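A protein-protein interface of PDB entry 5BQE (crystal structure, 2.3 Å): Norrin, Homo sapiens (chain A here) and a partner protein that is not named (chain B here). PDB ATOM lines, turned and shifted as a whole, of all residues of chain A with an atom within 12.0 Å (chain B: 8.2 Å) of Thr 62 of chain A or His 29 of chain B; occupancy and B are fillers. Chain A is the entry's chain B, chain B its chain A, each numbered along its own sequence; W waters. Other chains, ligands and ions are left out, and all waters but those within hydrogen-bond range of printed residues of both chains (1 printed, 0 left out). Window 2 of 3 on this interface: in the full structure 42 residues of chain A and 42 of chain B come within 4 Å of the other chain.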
ATOM      1  N   LEU A  57      -0.228 -16.682 -24.736  1.00  0.00           N
ATOM      2  CA  LEU A  57      -0.410 -17.785 -25.671  1.00  0.00           C
ATOM      3  C   LEU A  57       0.902 -18.556 -25.740  1.00  0.00           C
ATOM      4  O   LEU A  57       1.962 -17.998 -25.457  1.00  0.00           O
ATOM      5  CB  LEU A  57      -0.816 -17.282 -27.059  1.00  0.00           C
ATOM      6  CG  LEU A  57      -2.176 -16.593 -27.175  1.00  0.00           C
ATOM      7  CD1 LEU A  57      -2.299 -15.914 -28.530  1.00  0.00           C
ATOM      8  CD2 LEU A  57      -3.316 -17.584 -26.968  1.00  0.00           C
ATOM      9  N   VAL A  58       0.829 -19.832 -26.101  1.00  0.00           N
ATOM     10  CA  VAL A  58       2.021 -20.665 -26.207  1.00  0.00           C
ATOM     11  C   VAL A  58       2.357 -20.940 -27.667  1.00  0.00           C
ATOM     12  O   VAL A  58       1.517 -21.432 -28.421  1.00  0.00           O
ATOM     13  CB  VAL A  58       1.845 -22.009 -25.475  1.00  0.00           C
ATOM     14  CG1 VAL A  58       3.178 -22.742 -25.381  1.00  0.00           C
ATOM     15  CG2 VAL A  58       1.268 -21.788 -24.086  1.00  0.00           C
ATOM     16  N   SER A  59       3.584 -20.607 -28.060  1.00  0.00           N
ATOM     17  CA  SER A  59       4.070 -20.898 -29.405  1.00  0.00           C
ATOM     18  C   SER A  59       4.860 -22.200 -29.446  1.00  0.00           C
ATOM     19  O   SER A  59       5.479 -22.595 -28.459  1.00  0.00           O
ATOM     20  CB  SER A  59       4.953 -19.757 -29.924  1.00  0.00           C
ATOM     21  OG  SER A  59       4.189 -18.778 -30.605  1.00  0.00           O
ATOM     22  N   PHE A  60       4.828 -22.852 -30.603  1.00  0.00           N
ATOM     23  CA  PHE A  60       5.669 -24.010 -30.880  1.00  0.00           C
ATOM     24  C   PHE A  60       6.342 -23.781 -32.221  1.00  0.00           C
ATOM     25  O   PHE A  60       6.036 -22.811 -32.914  1.00  0.00           O
ATOM     26  CB  PHE A  60       4.852 -25.303 -30.899  1.00  0.00           C
ATOM     27  CG  PHE A  60       4.344 -25.724 -29.550  1.00  0.00           C
ATOM     28  CD1 PHE A  60       5.102 -26.544 -28.734  1.00  0.00           C
ATOM     29  CD2 PHE A  60       3.103 -25.306 -29.102  1.00  0.00           C
ATOM     30  CE1 PHE A  60       4.633 -26.935 -27.494  1.00  0.00           C
ATOM     31  CE2 PHE A  60       2.631 -25.694 -27.862  1.00  0.00           C
ATOM     32  CZ  PHE A  60       3.396 -26.511 -27.060  1.00  0.00           C
ATOM     33  N   SER A  61       7.230 -24.671 -32.596  1.00  0.00           N
ATOM     34  CA  SER A  61       7.845 -24.603 -33.889  1.00  0.00           C
ATOM     35  C   SER A  61       6.808 -24.521 -34.982  1.00  0.00           C
ATOM     36  O   SER A  61       6.982 -23.827 -35.940  1.00  0.00           O
ATOM     37  CB  SER A  61       8.717 -25.814 -34.102  1.00  0.00           C
ATOM     38  OG  SER A  61       9.895 -25.705 -33.374  1.00  0.00           O
ATOM     39  N   THR A  62       5.721 -25.240 -34.822  1.00  0.00           N
ATOM     40  CA  THR A  62       4.709 -25.284 -35.836  1.00  0.00           C
ATOM     41  C   THR A  62       3.496 -24.501 -35.468  1.00  0.00           C
ATOM     42  O   THR A  62       2.529 -24.517 -36.177  1.00  0.00           O
ATOM     43  CB  THR A  62       4.267 -26.711 -36.086  1.00  0.00           C
ATOM     44  OG1 THR A  62       4.072 -27.351 -34.834  1.00  0.00           O
ATOM     45  CG2 THR A  62       5.319 -27.424 -36.832  1.00  0.00           C
ATOM     46  N   VAL A  63       3.553 -23.821 -34.346  1.00  0.00           N
ATOM     47  CA  VAL A  63       2.433 -22.996 -33.899  1.00  0.00           C
ATOM     48  C   VAL A  63       2.901 -21.564 -33.657  1.00  0.00           C
ATOM     49  O   VAL A  63       3.415 -21.247 -32.583  1.00  0.00           O
ATOM     50  CB  VAL A  63       1.794 -23.568 -32.611  1.00  0.00           C
ATOM     51  CG1 VAL A  63       0.522 -22.815 -32.239  1.00  0.00           C
ATOM     52  CG2 VAL A  63       1.481 -25.046 -32.796  1.00  0.00           C
ATOM     53  N   LEU A  64       2.733 -20.711 -34.665  1.00  0.00           N
ATOM     54  CA  LEU A  64       3.076 -19.296 -34.549  1.00  0.00           C
ATOM     55  C   LEU A  64       1.948 -18.516 -33.872  1.00  0.00           C
ATOM     56  O   LEU A  64       0.862 -18.364 -34.440  1.00  0.00           O
ATOM     57  CB  LEU A  64       3.364 -18.683 -35.927  1.00  0.00           C
ATOM     58  CG  LEU A  64       4.554 -19.181 -36.753  1.00  0.00           C
ATOM     59  CD1 LEU A  64       5.109 -18.036 -37.591  1.00  0.00           C
ATOM     60  CD2 LEU A  64       5.635 -19.762 -35.891  1.00  0.00           C
ATOM     61  N   MLY A  65       2.209 -18.022 -32.663  1.00  0.00           N
ATOM     62  CA  MLY A  65       1.212 -17.247 -31.927  1.00  0.00           C
ATOM     63  CB  MLY A  65       0.572 -18.100 -30.829  1.00  0.00           C
ATOM     64  CG  MLY A  65      -0.595 -18.907 -31.354  1.00  0.00           C
ATOM     65  CD  MLY A  65      -1.151 -19.861 -30.320  1.00  0.00           C
ATOM     66  CE  MLY A  65      -2.301 -20.669 -30.903  1.00  0.00           C
ATOM     67  NZ  MLY A  65      -2.819 -21.677 -29.936  1.00  0.00           N
ATOM     68  CH1 MLY A  65      -4.024 -21.113 -29.311  1.00  0.00           C
ATOM     69  CH2 MLY A  65      -3.254 -22.837 -30.722  1.00  0.00           C
ATOM     70  C   MLY A  65       1.774 -15.950 -31.354  1.00  0.00           C
ATOM     71  O   MLY A  65       2.972 -15.833 -31.091  1.00  0.00           O
ATOM     72  N   GLN A  66       0.889 -14.972 -31.188  1.00  0.00           N
ATOM     73  CA  GLN A  66       1.235 -13.703 -30.568  1.00  0.00           C
ATOM     74  C   GLN A  66       1.493 -13.933 -29.089  1.00  0.00           C
ATOM     75  O   GLN A  66       1.020 -14.920 -28.535  1.00  0.00           O
ATOM     76  CB  GLN A  66       0.111 -12.687 -30.767  1.00  0.00           C
ATOM     77  CG  GLN A  66      -0.086 -12.276 -32.211  1.00  0.00           C
ATOM     78  CD  GLN A  66       1.084 -11.477 -32.743  1.00  0.00           C
ATOM     79  OE1 GLN A  66       1.484 -10.476 -32.152  1.00  0.00           O
ATOM     80  NE2 GLN A  66       1.646 -11.920 -33.861  1.00  0.00           N
ATOM     81  N   SER B  26      -2.252 -26.353 -18.422  1.00  0.00           N
ATOM     82  CA  SER B  26      -1.402 -27.390 -18.992  1.00  0.00           C
ATOM     83  C   SER B  26      -0.802 -26.943 -20.320  1.00  0.00           C
ATOM     84  O   SER B  26      -1.514 -26.450 -21.196  1.00  0.00           O
ATOM     85  CB  SER B  26      -2.201 -28.680 -19.192  1.00  0.00           C
ATOM     86  OG  SER B  26      -1.372 -29.821 -19.043  1.00  0.00           O
ATOM     87  N   ILE B  27       0.510 -27.112 -20.459  1.00  0.00           N
ATOM     88  CA  ILE B  27       1.187 -26.869 -21.727  1.00  0.00           C
ATOM     89  C   ILE B  27       1.214 -28.155 -22.543  1.00  0.00           C
ATOM     90  O   ILE B  27       1.875 -29.120 -22.161  1.00  0.00           O
ATOM     91  CB  ILE B  27       2.639 -26.385 -21.539  1.00  0.00           C
ATOM     92  CG1 ILE B  27       2.715 -25.212 -20.557  1.00  0.00           C
ATOM     93  CG2 ILE B  27       3.237 -25.986 -22.885  1.00  0.00           C
ATOM     94  CD1 ILE B  27       2.142 -23.915 -21.094  1.00  0.00           C
ATOM     95  N   SER B  28       0.502 -28.165 -23.664  1.00  0.00           N
ATOM     96  CA  SER B  28       0.498 -29.315 -24.560  1.00  0.00           C
ATOM     97  C   SER B  28       0.555 -28.843 -26.003  1.00  0.00           C
ATOM     98  O   SER B  28       0.025 -27.784 -26.337  1.00  0.00           O
ATOM     99  CB  SER B  28      -0.750 -30.172 -24.340  1.00  0.00           C
ATOM    100  OG  SER B  28      -1.912 -29.495 -24.786  1.00  0.00           O
ATOM    101  N   HIS B  29       1.150 -29.636 -26.871  1.00  0.00           N
ATOM    102  CA  HIS B  29       1.144 -29.303 -28.278  1.00  0.00           C
ATOM    103  C   HIS B  29      -0.216 -29.541 -28.838  1.00  0.00           C
ATOM    104  O   HIS B  29      -0.779 -30.571 -28.615  1.00  0.00           O
ATOM    105  CB  HIS B  29       2.133 -30.154 -29.016  1.00  0.00           C
ATOM    106  CG  HIS B  29       2.486 -29.619 -30.354  1.00  0.00           C
ATOM    107  ND1 HIS B  29       1.591 -29.579 -31.391  1.00  0.00           N
ATOM    108  CD2 HIS B  29       3.633 -29.095 -30.821  1.00  0.00           C
ATOM    109  CE1 HIS B  29       2.177 -29.057 -32.445  1.00  0.00           C
ATOM    110  NE2 HIS B  29       3.414 -28.752 -32.124  1.00  0.00           N
ATOM    111  N   PRO B  30      -0.767 -28.585 -29.552  1.00  0.00           N
ATOM    112  CA  PRO B  30      -2.158 -28.728 -29.996  1.00  0.00           C
ATOM    113  C   PRO B  30      -2.370 -29.867 -30.997  1.00  0.00           C
ATOM    114  O   PRO B  30      -3.518 -30.170 -31.323  1.00  0.00           O
ATOM    115  CB  PRO B  30      -2.453 -27.369 -30.643  1.00  0.00           C
ATOM    116  CG  PRO B  30      -1.128 -26.886 -31.108  1.00  0.00           C
ATOM    117  CD  PRO B  30      -0.164 -27.334 -30.048  1.00  0.00           C
ATOM    118  N   LEU B  31      -1.287 -30.485 -31.464  1.00  0.00           N
ATOM    119  CA  LEU B  31      -1.375 -31.589 -32.413  1.00  0.00           C
ATOM    120  C   LEU B  31      -0.462 -32.755 -32.025  1.00  0.00           C
ATOM    121  O   LEU B  31      -0.947 -33.850 -31.729  1.00  0.00           O
ATOM    122  CB  LEU B  31      -1.037 -31.104 -33.824  1.00  0.00           C
ATOM    123  CG  LEU B  31      -1.034 -32.175 -34.920  1.00  0.00           C
ATOM    124  CD1 LEU B  31      -1.501 -31.588 -36.244  1.00  0.00           C
ATOM    125  CD2 LEU B  31       0.342 -32.796 -35.082  1.00  0.00           C
ATOM    126  N   TYR B  32       0.832 -32.564 -32.142  1.00  0.00           N
ATOM    127  CA  TYR B  32       1.714 -33.661 -31.887  1.00  0.00           C
ATOM    128  C   TYR B  32       1.340 -34.234 -30.557  1.00  0.00           C
ATOM    129  O   TYR B  32       0.562 -33.646 -29.844  1.00  0.00           O
ATOM    130  CB  TYR B  32       3.158 -33.205 -31.923  1.00  0.00           C
ATOM    131  CG  TYR B  32       3.601 -32.748 -33.285  1.00  0.00           C
ATOM    132  CD1 TYR B  32       2.880 -33.059 -34.416  1.00  0.00           C
ATOM    133  CD2 TYR B  32       4.740 -32.012 -33.438  1.00  0.00           C
ATOM    134  CE1 TYR B  32       3.286 -32.644 -35.660  1.00  0.00           C
ATOM    135  CE2 TYR B  32       5.160 -31.592 -34.680  1.00  0.00           C
ATOM    136  CZ  TYR B  32       4.426 -31.908 -35.787  1.00  0.00           C
ATOM    137  OH  TYR B  32       4.844 -31.499 -37.025  1.00  0.00           O
ATOM    138  N   LYS B  33       1.877 -35.400 -30.238  1.00  0.00           N
ATOM    139  CA  LYS B  33       1.476 -36.094 -29.037  1.00  0.00           C
ATOM    140  C   LYS B  33       2.592 -36.077 -28.029  1.00  0.00           C
ATOM    141  O   LYS B  33       3.635 -36.656 -28.250  1.00  0.00           O
ATOM    142  CB  LYS B  33       1.103 -37.526 -29.387  1.00  0.00           C
ATOM    143  CG  LYS B  33      -0.359 -37.693 -29.779  1.00  0.00           C
ATOM    144  CD  LYS B  33      -0.570 -37.832 -31.279  1.00  0.00           C
ATOM    145  CE  LYS B  33       0.369 -36.947 -32.083  1.00  0.00           C
ATOM    146  NZ  LYS B  33       0.277 -37.216 -33.531  1.00  0.00           N
ATOM    147  N   CYS B  34       2.342 -35.445 -26.896  1.00  0.00           N
ATOM    148  CA  CYS B  34       3.401 -35.092 -25.987  1.00  0.00           C
ATOM    149  C   CYS B  34       3.100 -35.199 -24.524  1.00  0.00           C
ATOM    150  O   CYS B  34       1.984 -35.322 -24.098  1.00  0.00           O
ATOM    151  CB  CYS B  34       3.848 -33.678 -26.246  1.00  0.00           C
ATOM    152  SG  CYS B  34       4.344 -33.394 -27.928  1.00  0.00           S
ATOM    153  N   SER B  35       4.167 -35.145 -23.768  1.00  0.00           N
ATOM    154  CA  SER B  35       4.141 -35.085 -22.344  1.00  0.00           C
ATOM    155  C   SER B  35       3.732 -33.713 -21.822  1.00  0.00           C
ATOM    156  O   SER B  35       4.562 -32.870 -21.599  1.00  0.00           O
ATOM    157  CB  SER B  35       5.551 -35.366 -21.901  1.00  0.00           C
ATOM    158  OG  SER B  35       6.391 -35.255 -23.037  1.00  0.00           O
ATOM    159  N   SER B  36       2.446 -33.512 -21.588  1.00  0.00           N
ATOM    160  CA  SER B  36       1.935 -32.270 -21.015  1.00  0.00           C
ATOM    161  C   SER B  36       2.687 -31.897 -19.741  1.00  0.00           C
ATOM    162  O   SER B  36       3.214 -32.766 -19.047  1.00  0.00           O
ATOM    163  CB  SER B  36       0.441 -32.397 -20.721  1.00  0.00           C
ATOM    164  OG  SER B  36      -0.319 -32.358 -21.916  1.00  0.00           O
ATOM    165  N   LYS B  37       2.733 -30.602 -19.440  1.00  0.00           N
ATOM    166  CA  LYS B  37       3.448 -30.113 -18.267  1.00  0.00           C
ATOM    167  C   LYS B  37       2.642 -29.034 -17.557  1.00  0.00           C
ATOM    168  O   LYS B  37       2.137 -28.101 -18.186  1.00  0.00           O
ATOM    169  CB  LYS B  37       4.823 -29.575 -18.669  1.00  0.00           C
ATOM    170  CG  LYS B  37       5.930 -29.854 -17.665  1.00  0.00           C
ATOM    171  CD  LYS B  37       7.218 -30.212 -18.385  1.00  0.00           C
ATOM    172  CE  LYS B  37       8.426 -30.132 -17.470  1.00  0.00           C
ATOM    173  NZ  LYS B  37       9.685 -30.434 -18.205  1.00  0.00           N
ATOM    174  N   LEU B  87       9.097 -30.147 -23.998  1.00  0.00           N
ATOM    175  CA  LEU B  87       8.224 -31.306 -23.859  1.00  0.00           C
ATOM    176  C   LEU B  87       8.859 -32.531 -24.508  1.00  0.00           C
ATOM    177  O   LEU B  87       9.555 -32.412 -25.514  1.00  0.00           O
ATOM    178  CB  LEU B  87       6.862 -31.035 -24.502  1.00  0.00           C
ATOM    179  CG  LEU B  87       6.075 -29.816 -24.017  1.00  0.00           C
ATOM    180  CD1 LEU B  87       4.672 -29.826 -24.613  1.00  0.00           C
ATOM    181  CD2 LEU B  87       6.017 -29.766 -22.501  1.00  0.00           C
ATOM    182  N   CYS B  89       8.048 -35.558 -26.623  1.00  0.00           N
ATOM    183  CA  CYS B  89       6.962 -35.995 -27.458  1.00  0.00           C
ATOM    184  C   CYS B  89       7.175 -37.423 -27.896  1.00  0.00           C
ATOM    185  O   CYS B  89       8.108 -38.039 -27.435  1.00  0.00           O
ATOM    186  CB  CYS B  89       6.749 -35.005 -28.576  1.00  0.00           C
ATOM    187  SG  CYS B  89       6.325 -33.439 -27.821  1.00  0.00           S
ATOM    188  N   LEU B  95      10.465 -30.853 -27.927  1.00  0.00           N
ATOM    189  CA  LEU B  95       9.914 -29.658 -28.546  1.00  0.00           C
ATOM    190  C   LEU B  95       9.917 -28.480 -27.615  1.00  0.00           C
ATOM    191  O   LEU B  95       9.458 -28.588 -26.509  1.00  0.00           O
ATOM    192  CB  LEU B  95       8.481 -29.902 -28.947  1.00  0.00           C
ATOM    193  CG  LEU B  95       8.305 -30.920 -30.043  1.00  0.00           C
ATOM    194  CD1 LEU B  95       6.908 -30.841 -30.593  1.00  0.00           C
ATOM    195  CD2 LEU B  95       9.329 -30.709 -31.133  1.00  0.00           C
ATOM    196  N   THR B  96      10.425 -27.359 -28.085  1.00  0.00           N
ATOM    197  CA  THR B  96      10.488 -26.124 -27.314  1.00  0.00           C
ATOM    198  C   THR B  96       9.171 -25.363 -27.400  1.00  0.00           C
ATOM    199  O   THR B  96       8.684 -25.075 -28.493  1.00  0.00           O
ATOM    200  CB  THR B  96      11.623 -25.212 -27.813  1.00  0.00           C
ATOM    201  OG1 THR B  96      12.883 -25.867 -27.629  1.00  0.00           O
ATOM    202  CG2 THR B  96      11.629 -23.879 -27.065  1.00  0.00           C
ATOM    203  N   ALA B  97       8.612 -25.026 -26.243  1.00  0.00           N
ATOM    204  CA  ALA B  97       7.439 -24.161 -26.177  1.00  0.00           C
ATOM    205  C   ALA B  97       7.842 -22.857 -25.519  1.00  0.00           C
ATOM    206  O   ALA B  97       8.641 -22.856 -24.582  1.00  0.00           O
ATOM    207  CB  ALA B  97       6.316 -24.821 -25.406  1.00  0.00           C
HETATM  208  O   HOH W   1       8.236 -26.651 -30.825  1.00  0.00           O
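Thr 62 of chain A touches just one residue of chain B: His 29.
Of chain A, only Phe 60 (3.6 Å) and Thr 62 (3.1 Å) come within 4 Å of His 29 of chain B.
Pro 30 of chain B touches just these residues of chain A: Phe 60 and Val 63.
No residue of chain A comes within 4 Å of Leu 31 of chain B.
Cys 34 of chain B touches none of the printed residues of chain A.
No residue of chain A comes within 4 Å of Leu 95 of chain B.
Of the printed residues of chain B, Val 63 of chain A touches Pro 30.
Printed residues of chain A within 4 Å of Ala 97 of chain B: Val 58, Ser 59 and Phe 60.
The nearest residue of chain B that does not touch Thr 62 of chain A is Tyr 32 of chain B (4.1 Å).
The nearest residue of chain A that does not touch His 29 of chain B is Val 63 of chain A (4.1 Å).
The nearest printed residue of chain B that does not touch Ser 59 of chain A is Thr 96 of chain B (4.1 Å).
Val 58 of chain A touches Ile 27 of chain B.
Val 58 of chain A touches Ala 97 of chain B.
CA of Ala 97 of chain B touches O of Ser 59 of chain A, at 3.4 Å.
Ser 28 of chain B touches Phe 60 of chain A (O to CE2, 3.7 Å).
His 29 of chain B touches Phe 60 of chain A (CD2 to CD1, 3.6 Å).
Pro 30 of chain B touches Phe 60 of chain A (CD to CE2, 3.9 Å).
Thr 96 of chain B touches Phe 60 of chain A (O to CD1, 3.9 Å).
Ala 97 of chain B touches Phe 60 of chain A (CB to CE1, 3.4 Å).
Pro 30 of chain B touches Val 63 of chain A.
Of the 17 printed residues of chain B, 6 touch a printed residue of chain A.
Hydrophobic or aromatic side chains of chain B within 4 Å of the printed part of chain A: Ile 27, His 29, Pro 30 and Ala 97.
Of the 10 printed residues of chain A, 5 touch a printed residue of chain B.
Hydrophobic or aromatic side chains of chain A within 4 Å of the printed part of chain B: Val 58, Phe 60 and Val 63.
Among the printed residues, no Asp or Glu carboxylate lies within 4 Å of a Lys or Arg side-chain nitrogen of the other chain.
NE2 of His 29 of chain B lies within hydrogen-bond range of OG1 of Thr 62 of chain A, at 3.1 Å.
N of MLY 65 of chain A sits at hydrogen-bond distance from OG of Ser 59 of chain A, 3.0 Å away.
The backbone NH of Ile 27 of chain B sits at hydrogen-bond distance from the backbone carbonyl oxygen of Lys 37 of chain B, 3.0 Å away.
A ring nitrogen (ND1) of His 29 of chain B lies close to the backbone NH (N) of Leu 31 of chain B, 3.0 Å away.
ND1 of His 29 of chain B lies within hydrogen-bond range of N of Tyr 32 of chain B (3.2 Å).
The side-chain hydroxyl (OG) of Ser 59 of chain A is in hydrogen-bond range of the backbone carbonyl oxygen (O) of Val 63 of chain A, 3.3 Å away.
The side-chain sulfur of Cys 34 of chain B is disulfide-bonded to the side-chain sulfur of Cys 89 of chain B (2.0 Å).
Water W1 lies within hydrogen-bond range of the backbone NH (N) of Ser 61 of chain A and the backbone carbonyl oxygen (O) of Thr 96 of chain B.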
